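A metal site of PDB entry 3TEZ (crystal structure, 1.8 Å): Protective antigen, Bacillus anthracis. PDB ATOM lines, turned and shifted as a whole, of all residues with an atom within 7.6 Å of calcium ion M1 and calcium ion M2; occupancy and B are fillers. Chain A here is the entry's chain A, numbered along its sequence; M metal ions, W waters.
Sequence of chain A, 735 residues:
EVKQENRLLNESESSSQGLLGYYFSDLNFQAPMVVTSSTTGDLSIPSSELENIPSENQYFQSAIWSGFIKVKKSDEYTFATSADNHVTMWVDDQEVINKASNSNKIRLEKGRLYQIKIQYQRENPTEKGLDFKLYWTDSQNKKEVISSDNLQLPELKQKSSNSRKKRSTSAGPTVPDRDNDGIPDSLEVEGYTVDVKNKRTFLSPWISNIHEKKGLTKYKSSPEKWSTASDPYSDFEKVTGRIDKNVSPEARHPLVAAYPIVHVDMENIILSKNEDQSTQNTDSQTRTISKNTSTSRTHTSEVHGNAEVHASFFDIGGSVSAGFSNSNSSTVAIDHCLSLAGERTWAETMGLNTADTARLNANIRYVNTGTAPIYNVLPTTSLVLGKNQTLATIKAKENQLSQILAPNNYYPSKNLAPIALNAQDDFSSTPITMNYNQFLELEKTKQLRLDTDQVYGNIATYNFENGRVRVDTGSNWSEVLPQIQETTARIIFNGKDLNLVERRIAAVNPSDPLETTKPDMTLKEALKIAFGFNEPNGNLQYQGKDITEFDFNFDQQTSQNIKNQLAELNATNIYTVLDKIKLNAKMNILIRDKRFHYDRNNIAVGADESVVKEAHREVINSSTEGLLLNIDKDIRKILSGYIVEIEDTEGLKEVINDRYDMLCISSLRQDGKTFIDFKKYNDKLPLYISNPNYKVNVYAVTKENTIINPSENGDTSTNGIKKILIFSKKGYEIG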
ATOM      1  N   TYR A  22      20.299  16.189 -15.805  1.00  0.00           N
ATOM      2  CA  TYR A  22      19.380  17.297 -16.011  1.00  0.00           C
ATOM      3  C   TYR A  22      18.789  17.676 -14.659  1.00  0.00           C
ATOM      4  O   TYR A  22      18.229  16.823 -13.986  1.00  0.00           O
ATOM      5  CB  TYR A  22      18.251  16.868 -16.949  1.00  0.00           C
ATOM      6  CG  TYR A  22      18.751  16.460 -18.328  1.00  0.00           C
ATOM      7  CD1 TYR A  22      19.010  15.140 -18.624  1.00  0.00           C
ATOM      8  CD2 TYR A  22      18.982  17.416 -19.305  1.00  0.00           C
ATOM      9  CE1 TYR A  22      19.463  14.766 -19.864  1.00  0.00           C
ATOM     10  CE2 TYR A  22      19.452  17.046 -20.555  1.00  0.00           C
ATOM     11  CZ  TYR A  22      19.680  15.727 -20.822  1.00  0.00           C
ATOM     12  OH  TYR A  22      20.135  15.343 -22.063  1.00  0.00           O
ATOM     13  N   PRO A 176      12.218  15.930 -23.169  1.00  0.00           N
ATOM     14  CA  PRO A 176      12.129  16.119 -24.622  1.00  0.00           C
ATOM     15  C   PRO A 176      13.503  16.454 -25.226  1.00  0.00           C
ATOM     16  O   PRO A 176      14.127  17.433 -24.830  1.00  0.00           O
ATOM     17  CB  PRO A 176      11.151  17.302 -24.754  1.00  0.00           C
ATOM     18  CG  PRO A 176      10.324  17.248 -23.485  1.00  0.00           C
ATOM     19  CD  PRO A 176      11.282  16.784 -22.422  1.00  0.00           C
ATOM     20  N   ASP A 177      13.959  15.600 -26.130  1.00  0.00           N
ATOM     21  CA  ASP A 177      15.244  15.799 -26.825  1.00  0.00           C
ATOM     22  C   ASP A 177      15.082  15.170 -28.200  1.00  0.00           C
ATOM     23  O   ASP A 177      15.647  14.117 -28.464  1.00  0.00           O
ATOM     24  CB  ASP A 177      16.366  15.109 -26.046  1.00  0.00           C
ATOM     25  CG  ASP A 177      17.746  15.354 -26.659  1.00  0.00           C
ATOM     26  OD1 ASP A 177      17.875  16.260 -27.507  1.00  0.00           O
ATOM     27  OD2 ASP A 177      18.707  14.636 -26.316  1.00  0.00           O
ATOM     28  N   ARG A 178      14.288  15.809 -29.044  1.00  0.00           N
ATOM     29  CA  ARG A 178      13.840  15.248 -30.332  1.00  0.00           C
ATOM     30  C   ARG A 178      15.002  14.778 -31.240  1.00  0.00           C
ATOM     31  O   ARG A 178      14.901  13.752 -31.915  1.00  0.00           O
ATOM     32  CB  ARG A 178      12.905  16.259 -31.040  1.00  0.00           C
ATOM     33  CG  ARG A 178      11.626  16.567 -30.240  1.00  0.00           C
ATOM     34  CD  ARG A 178      10.849  17.775 -30.772  1.00  0.00           C
ATOM     35  NE  ARG A 178       9.993  17.447 -31.915  1.00  0.00           N
ATOM     36  CZ  ARG A 178       8.846  16.790 -31.831  1.00  0.00           C
ATOM     37  NH1 ARG A 178       8.417  16.354 -30.648  1.00  0.00           N
ATOM     38  NH2 ARG A 178       8.128  16.549 -32.919  1.00  0.00           N
ATOM     39  N   ASP A 179      16.120  15.504 -31.220  1.00  0.00           N
ATOM     40  CA  ASP A 179      17.248  15.158 -32.093  1.00  0.00           C
ATOM     41  C   ASP A 179      18.357  14.359 -31.403  1.00  0.00           C
ATOM     42  O   ASP A 179      19.371  14.045 -32.009  1.00  0.00           O
ATOM     43  CB  ASP A 179      17.850  16.427 -32.722  1.00  0.00           C
ATOM     44  CG  ASP A 179      18.252  17.445 -31.688  1.00  0.00           C
ATOM     45  OD1 ASP A 179      18.410  17.071 -30.504  1.00  0.00           O
ATOM     46  OD2 ASP A 179      18.358  18.626 -32.070  1.00  0.00           O
ATOM     47  N   ASN A 180      18.168  14.019 -30.131  1.00  0.00           N
ATOM     48  CA  ASN A 180      19.143  13.210 -29.412  1.00  0.00           C
ATOM     49  C   ASN A 180      20.518  13.851 -29.289  1.00  0.00           C
ATOM     50  O   ASN A 180      21.533  13.140 -29.217  1.00  0.00           O
ATOM     51  CB  ASN A 180      19.268  11.787 -30.005  1.00  0.00           C
ATOM     52  CG  ASN A 180      19.822  10.760 -29.004  1.00  0.00           C
ATOM     53  OD1 ASN A 180      19.286  10.791 -27.788  1.00  0.00           O
ATOM     54  ND2 ASN A 180      20.713   9.973 -29.306  1.00  0.00           N
ATOM     55  N   ASP A 181      20.595  15.186 -29.262  1.00  0.00           N
ATOM     56  CA  ASP A 181      21.949  15.739 -29.110  1.00  0.00           C
ATOM     57  C   ASP A 181      22.292  15.951 -27.640  1.00  0.00           C
ATOM     58  O   ASP A 181      23.447  16.194 -27.290  1.00  0.00           O
ATOM     59  CB  ASP A 181      22.193  17.007 -29.953  1.00  0.00           C
ATOM     60  CG  ASP A 181      21.283  18.155 -29.592  1.00  0.00           C
ATOM     61  OD1 ASP A 181      20.686  18.190 -28.481  1.00  0.00           O
ATOM     62  OD2 ASP A 181      21.201  19.088 -30.428  1.00  0.00           O
ATOM     63  N   GLY A 182      21.293  15.823 -26.787  1.00  0.00           N
ATOM     64  CA  GLY A 182      21.515  15.991 -25.362  1.00  0.00           C
ATOM     65  C   GLY A 182      20.989  17.291 -24.800  1.00  0.00           C
ATOM     66  O   GLY A 182      20.811  17.418 -23.596  1.00  0.00           O
ATOM     67  N   ILE A 183      20.742  18.281 -25.651  1.00  0.00           N
ATOM     68  CA  ILE A 183      20.174  19.547 -25.178  1.00  0.00           C
ATOM     69  C   ILE A 183      18.664  19.479 -25.272  1.00  0.00           C
ATOM     70  O   ILE A 183      18.115  19.284 -26.353  1.00  0.00           O
ATOM     71  CB  ILE A 183      20.682  20.765 -25.971  1.00  0.00           C
ATOM     72  CG1 ILE A 183      22.222  20.749 -26.107  1.00  0.00           C
ATOM     73  CG2 ILE A 183      20.133  22.085 -25.318  1.00  0.00           C
ATOM     74  CD1 ILE A 183      22.816  21.782 -27.097  1.00  0.00           C
ATOM     75  N   PRO A 184      17.960  19.654 -24.143  1.00  0.00           N
ATOM     76  CA  PRO A 184      16.488  19.587 -24.108  1.00  0.00           C
ATOM     77  C   PRO A 184      15.847  20.526 -25.136  1.00  0.00           C
ATOM     78  O   PRO A 184      16.333  21.642 -25.313  1.00  0.00           O
ATOM     79  CB  PRO A 184      16.162  20.050 -22.692  1.00  0.00           C
ATOM     80  CG  PRO A 184      17.389  19.668 -21.886  1.00  0.00           C
ATOM     81  CD  PRO A 184      18.538  19.913 -22.818  1.00  0.00           C
ATOM     82  N   ASP A 185      14.763  20.100 -25.790  1.00  0.00           N
ATOM     83  CA  ASP A 185      14.089  20.938 -26.794  1.00  0.00           C
ATOM     84  C   ASP A 185      13.928  22.392 -26.331  1.00  0.00           C
ATOM     85  O   ASP A 185      14.201  23.333 -27.078  1.00  0.00           O
ATOM     86  CB  ASP A 185      12.672  20.432 -27.096  1.00  0.00           C
ATOM     87  CG  ASP A 185      12.640  19.038 -27.707  1.00  0.00           C
ATOM     88  OD1 ASP A 185      13.689  18.390 -27.899  1.00  0.00           O
ATOM     89  OD2 ASP A 185      11.495  18.576 -27.969  1.00  0.00           O
ATOM     90  N   SER A 186      13.424  22.573 -25.119  1.00  0.00           N
ATOM     91  CA  SER A 186      13.044  23.898 -24.642  1.00  0.00           C
ATOM     92  C   SER A 186      14.231  24.850 -24.570  1.00  0.00           C
ATOM     93  O   SER A 186      14.087  26.044 -24.847  1.00  0.00           O
ATOM     94  CB  SER A 186      12.329  23.832 -23.286  1.00  0.00           C
ATOM     95  OG  SER A 186      13.154  23.292 -22.282  1.00  0.00           O
ATOM     96  N   GLU A 188      17.015  24.697 -26.437  1.00  0.00           N
ATOM     97  CA  GLU A 188      17.513  25.014 -27.778  1.00  0.00           C
ATOM     98  C   GLU A 188      16.674  26.123 -28.419  1.00  0.00           C
ATOM     99  O   GLU A 188      17.187  26.999 -29.124  1.00  0.00           O
ATOM    100  CB  GLU A 188      17.509  23.765 -28.665  1.00  0.00           C
ATOM    101  CG  GLU A 188      18.521  22.716 -28.274  1.00  0.00           C
ATOM    102  CD  GLU A 188      18.896  21.807 -29.404  1.00  0.00           C
ATOM    103  OE1 GLU A 188      19.607  22.238 -30.343  1.00  0.00           O
ATOM    104  OE2 GLU A 188      18.481  20.644 -29.390  1.00  0.00           O
ATOM    105  N   TYR A 192      20.069  29.396 -24.533  1.00  0.00           N
ATOM    106  CA  TYR A 192      20.870  28.836 -23.456  1.00  0.00           C
ATOM    107  C   TYR A 192      22.272  29.437 -23.426  1.00  0.00           C
ATOM    108  O   TYR A 192      22.745  30.034 -24.403  1.00  0.00           O
ATOM    109  CB  TYR A 192      20.979  27.298 -23.552  1.00  0.00           C
ATOM    110  CG  TYR A 192      21.470  26.743 -24.884  1.00  0.00           C
ATOM    111  CD1 TYR A 192      20.619  26.658 -25.974  1.00  0.00           C
ATOM    112  CD2 TYR A 192      22.765  26.267 -25.028  1.00  0.00           C
ATOM    113  CE1 TYR A 192      21.046  26.133 -27.180  1.00  0.00           C
ATOM    114  CE2 TYR A 192      23.224  25.739 -26.240  1.00  0.00           C
ATOM    115  CZ  TYR A 192      22.352  25.669 -27.320  1.00  0.00           C
ATOM    116  OH  TYR A 192      22.763  25.151 -28.528  1.00  0.00           O
ATOM    117  N   SER A 221      19.463  26.954 -30.989  1.00  0.00           N
ATOM    118  CA  SER A 221      19.750  25.948 -32.008  1.00  0.00           C
ATOM    119  C   SER A 221      18.444  25.200 -32.323  1.00  0.00           C
ATOM    120  O   SER A 221      17.453  25.401 -31.644  1.00  0.00           O
ATOM    121  CB  SER A 221      20.854  25.016 -31.526  1.00  0.00           C
ATOM    122  OG  SER A 221      20.634  24.604 -30.174  1.00  0.00           O
ATOM    123  N   SER A 222      18.438  24.379 -33.361  1.00  0.00           N
ATOM    124  CA  SER A 222      17.222  23.640 -33.682  1.00  0.00           C
ATOM    125  C   SER A 222      17.096  22.405 -32.804  1.00  0.00           C
ATOM    126  O   SER A 222      18.029  21.634 -32.718  1.00  0.00           O
ATOM    127  CB  SER A 222      17.192  23.165 -35.128  1.00  0.00           C
ATOM    128  OG  SER A 222      16.127  22.211 -35.256  1.00  0.00           O
ATOM    129  N   PRO A 223      15.925  22.213 -32.173  1.00  0.00           N
ATOM    130  CA  PRO A 223      15.674  21.017 -31.354  1.00  0.00           C
ATOM    131  C   PRO A 223      15.442  19.758 -32.194  1.00  0.00           C
ATOM    132  O   PRO A 223      15.337  18.670 -31.647  1.00  0.00           O
ATOM    133  CB  PRO A 223      14.417  21.392 -30.571  1.00  0.00           C
ATOM    134  CG  PRO A 223      13.679  22.314 -31.486  1.00  0.00           C
ATOM    135  CD  PRO A 223      14.781  23.138 -32.151  1.00  0.00           C
ATOM    136  N   GLU A 224      15.420  19.913 -33.521  1.00  0.00           N
ATOM    137  CA  GLU A 224      15.197  18.772 -34.419  1.00  0.00           C
ATOM    138  C   GLU A 224      16.379  18.494 -35.372  1.00  0.00           C
ATOM    139  O   GLU A 224      16.348  17.563 -36.194  1.00  0.00           O
ATOM    140  CB  GLU A 224      13.884  18.969 -35.165  1.00  0.00           C
ATOM    141  CG  GLU A 224      12.677  18.976 -34.205  1.00  0.00           C
ATOM    142  CD  GLU A 224      11.338  19.093 -34.909  1.00  0.00           C
ATOM    143  OE1 GLU A 224      11.306  18.892 -36.140  1.00  0.00           O
ATOM    144  OE2 GLU A 224      10.321  19.392 -34.232  1.00  0.00           O
ATOM    145  N   LYS A 225      17.433  19.291 -35.229  1.00  0.00           N
ATOM    146  CA  LYS A 225      18.667  19.020 -35.947  1.00  0.00           C
ATOM    147  C   LYS A 225      19.776  18.755 -34.946  1.00  0.00           C
ATOM    148  O   LYS A 225      20.141  19.637 -34.181  1.00  0.00           O
ATOM    149  CB  LYS A 225      19.026  20.212 -36.827  1.00  0.00           C
ATOM    150  CG  LYS A 225      17.948  20.586 -37.829  1.00  0.00           C
ATOM    151  CD  LYS A 225      18.460  21.662 -38.799  1.00  0.00           C
ATOM    152  CE  LYS A 225      19.447  21.089 -39.809  1.00  0.00           C
ATOM    153  NZ  LYS A 225      20.005  22.205 -40.600  1.00  0.00           N
ATOM    154  N   TRP A 226      20.308  17.548 -34.965  1.00  0.00           N
ATOM    155  CA  TRP A 226      21.394  17.132 -34.090  1.00  0.00           C
ATOM    156  C   TRP A 226      22.593  18.081 -34.266  1.00  0.00           C
ATOM    157  O   TRP A 226      23.191  18.518 -33.283  1.00  0.00           O
ATOM    158  CB  TRP A 226      21.735  15.678 -34.424  1.00  0.00           C
ATOM    159  CG  TRP A 226      22.903  15.053 -33.721  1.00  0.00           C
ATOM    160  CD1 TRP A 226      22.889  14.367 -32.537  1.00  0.00           C
ATOM    161  CD2 TRP A 226      24.257  14.998 -34.198  1.00  0.00           C
ATOM    162  NE1 TRP A 226      24.153  13.919 -32.230  1.00  0.00           N
ATOM    163  CE2 TRP A 226      25.015  14.293 -33.238  1.00  0.00           C
ATOM    164  CE3 TRP A 226      24.910  15.509 -35.328  1.00  0.00           C
ATOM    165  CZ2 TRP A 226      26.385  14.068 -33.370  1.00  0.00           C
ATOM    166  CZ3 TRP A 226      26.286  15.276 -35.474  1.00  0.00           C
ATOM    167  CH2 TRP A 226      27.008  14.572 -34.494  1.00  0.00           C
ATOM    168  N   SER A 227      22.947  18.382 -35.514  1.00  0.00           N
ATOM    169  CA  SER A 227      23.824  19.527 -35.819  1.00  0.00           C
ATOM    170  C   SER A 227      22.991  20.542 -36.572  1.00  0.00           C
ATOM    171  O   SER A 227      22.500  20.267 -37.669  1.00  0.00           O
ATOM    172  CB  SER A 227      25.034  19.124 -36.655  1.00  0.00           C
ATOM    173  OG  SER A 227      25.737  20.281 -37.093  1.00  0.00           O
ATOM    174  N   THR A 228      22.819  21.709 -35.983  1.00  0.00           N
ATOM    175  CA  THR A 228      21.949  22.718 -36.578  1.00  0.00           C
ATOM    176  C   THR A 228      22.550  23.289 -37.876  1.00  0.00           C
ATOM    177  O   THR A 228      21.809  23.647 -38.791  1.00  0.00           O
ATOM    178  CB  THR A 228      21.596  23.802 -35.561  1.00  0.00           C
ATOM    179  OG1 THR A 228      20.785  23.212 -34.534  1.00  0.00           O
ATOM    180  CG2 THR A 228      20.818  24.945 -36.204  1.00  0.00           C
ATOM    181  N   SER A 234      27.807  17.710 -33.119  1.00  0.00           N
ATOM    182  CA  SER A 234      26.490  18.015 -32.573  1.00  0.00           C
ATOM    183  C   SER A 234      26.433  19.362 -31.830  1.00  0.00           C
ATOM    184  O   SER A 234      27.463  19.890 -31.370  1.00  0.00           O
ATOM    185  CB  SER A 234      26.009  16.907 -31.643  1.00  0.00           C
ATOM    186  OG  SER A 234      26.227  17.253 -30.294  1.00  0.00           O
ATOM    187  N   ASP A 235      25.236  19.911 -31.710  1.00  0.00           N
ATOM    188  CA  ASP A 235      25.073  21.209 -31.031  1.00  0.00           C
ATOM    189  C   ASP A 235      25.658  21.136 -29.609  1.00  0.00           C
ATOM    190  O   ASP A 235      26.313  22.055 -29.124  1.00  0.00           O
ATOM    191  CB  ASP A 235      23.608  21.625 -31.005  1.00  0.00           C
ATOM    192  CG  ASP A 235      23.049  21.844 -32.380  1.00  0.00           C
ATOM    193  OD1 ASP A 235      23.793  22.139 -33.341  1.00  0.00           O
ATOM    194  OD2 ASP A 235      21.816  21.755 -32.512  1.00  0.00           O
ATOM    195  N   PHE A 236      25.437  19.997 -28.960  1.00  0.00           N
ATOM    196  CA  PHE A 236      25.950  19.750 -27.615  1.00  0.00           C
ATOM    197  C   PHE A 236      27.464  19.505 -27.586  1.00  0.00           C
ATOM    198  O   PHE A 236      28.172  20.043 -26.717  1.00  0.00           O
ATOM    199  CB  PHE A 236      25.169  18.559 -27.039  1.00  0.00           C
ATOM    200  CG  PHE A 236      25.614  18.122 -25.667  1.00  0.00           C
ATOM    201  CD1 PHE A 236      25.166  18.791 -24.539  1.00  0.00           C
ATOM    202  CD2 PHE A 236      26.451  17.021 -25.519  1.00  0.00           C
ATOM    203  CE1 PHE A 236      25.543  18.355 -23.267  1.00  0.00           C
ATOM    204  CE2 PHE A 236      26.834  16.597 -24.251  1.00  0.00           C
ATOM    205  CZ  PHE A 236      26.386  17.266 -23.123  1.00  0.00           C
ATOM    206  N   PRO A 254      26.709  26.567 -32.388  1.00  0.00           N
ATOM    207  CA  PRO A 254      25.845  25.651 -33.135  1.00  0.00           C
ATOM    208  C   PRO A 254      25.295  26.226 -34.445  1.00  0.00           C
ATOM    209  O   PRO A 254      24.853  25.435 -35.287  1.00  0.00           O
ATOM    210  CB  PRO A 254      24.695  25.372 -32.156  1.00  0.00           C
ATOM    211  CG  PRO A 254      25.294  25.562 -30.804  1.00  0.00           C
ATOM    212  CD  PRO A 254      26.283  26.702 -30.977  1.00  0.00           C
HETATM  213 CA    CA M   1      18.224  18.460 -28.509  1.00  0.00          CA
HETATM  214 CA    CA M   2      19.874  20.448 -31.854  1.00  0.00          CA
HETATM  215  O   HOH W   1      15.879  18.781 -29.134  1.00  0.00           O
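The backbone NH (N) of Lys 225 is in hydrogen-bond range of the side-chain hydroxyl (OG) of Ser 222 (3.2 Å). OG1 of Thr 228 lies within hydrogen-bond range of N of Ser 222 (2.9 Å). The side-chain hydroxyl of Ser 222 sits at hydrogen-bond distance from the backbone NH of Glu 224 (3.0 Å). N of Ser 221 lies within hydrogen-bond range of O of Glu 188, 2.9 Å away. O of Trp 226 is in hydrogen-bond range of N of Asp 235. The side-chain carboxylate (OD2) of Asp 177 lies within hydrogen-bond range of the backbone NH (N) of Gly 182, 2.9 Å away. The backbone NH (N) of Asp 177 sits close to the side-chain carboxylate (OD1) of Asp 185, at 3.3 Å. The backbone NH (N) of Asn 180 lies close to the side-chain carboxylate (OD1) of Asp 177 (3.5 Å).
The nearest printed residue that does not touch calcium ion M1 is Pro 223 (4.3 Å).
Residues that only touch calcium ion M2: Thr 228.
Calcium ion M1 is bound by the backbone carbonyl oxygen (O) of Ile 183 (2.3 Å), the side-chain carboxylate (OE2) of Glu 188 (2.4 Å), the side-chain carboxylate (OD1) of Asp 179 (2.4 Å), the side-chain carboxylate (OD1) of Asp 177 (2.4 Å), water W1 (2.4 Å) and the side-chain carboxylate (OD1) of Asp 181 (2.5 Å).
Calcium ion M2 is bound by O of Ser 222 (2.4 Å), OE1 of Glu 188 (2.4 Å), OD2 of Asp 181 (2.4 Å), OD2 of Asp 179 (2.4 Å), OD2 of Asp 235 (2.4 Å), O of Lys 225 (2.5 Å) and OE2 of Glu 188 (2.8 Å). Calcium ion M2 has seven donor atoms within binding distance.
Water W1 lies within hydrogen-bond range of OD1 of Asp 185 (2.5 Å), O of Pro 223 (2.6 Å) and N of Arg 178 (3.4 Å).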
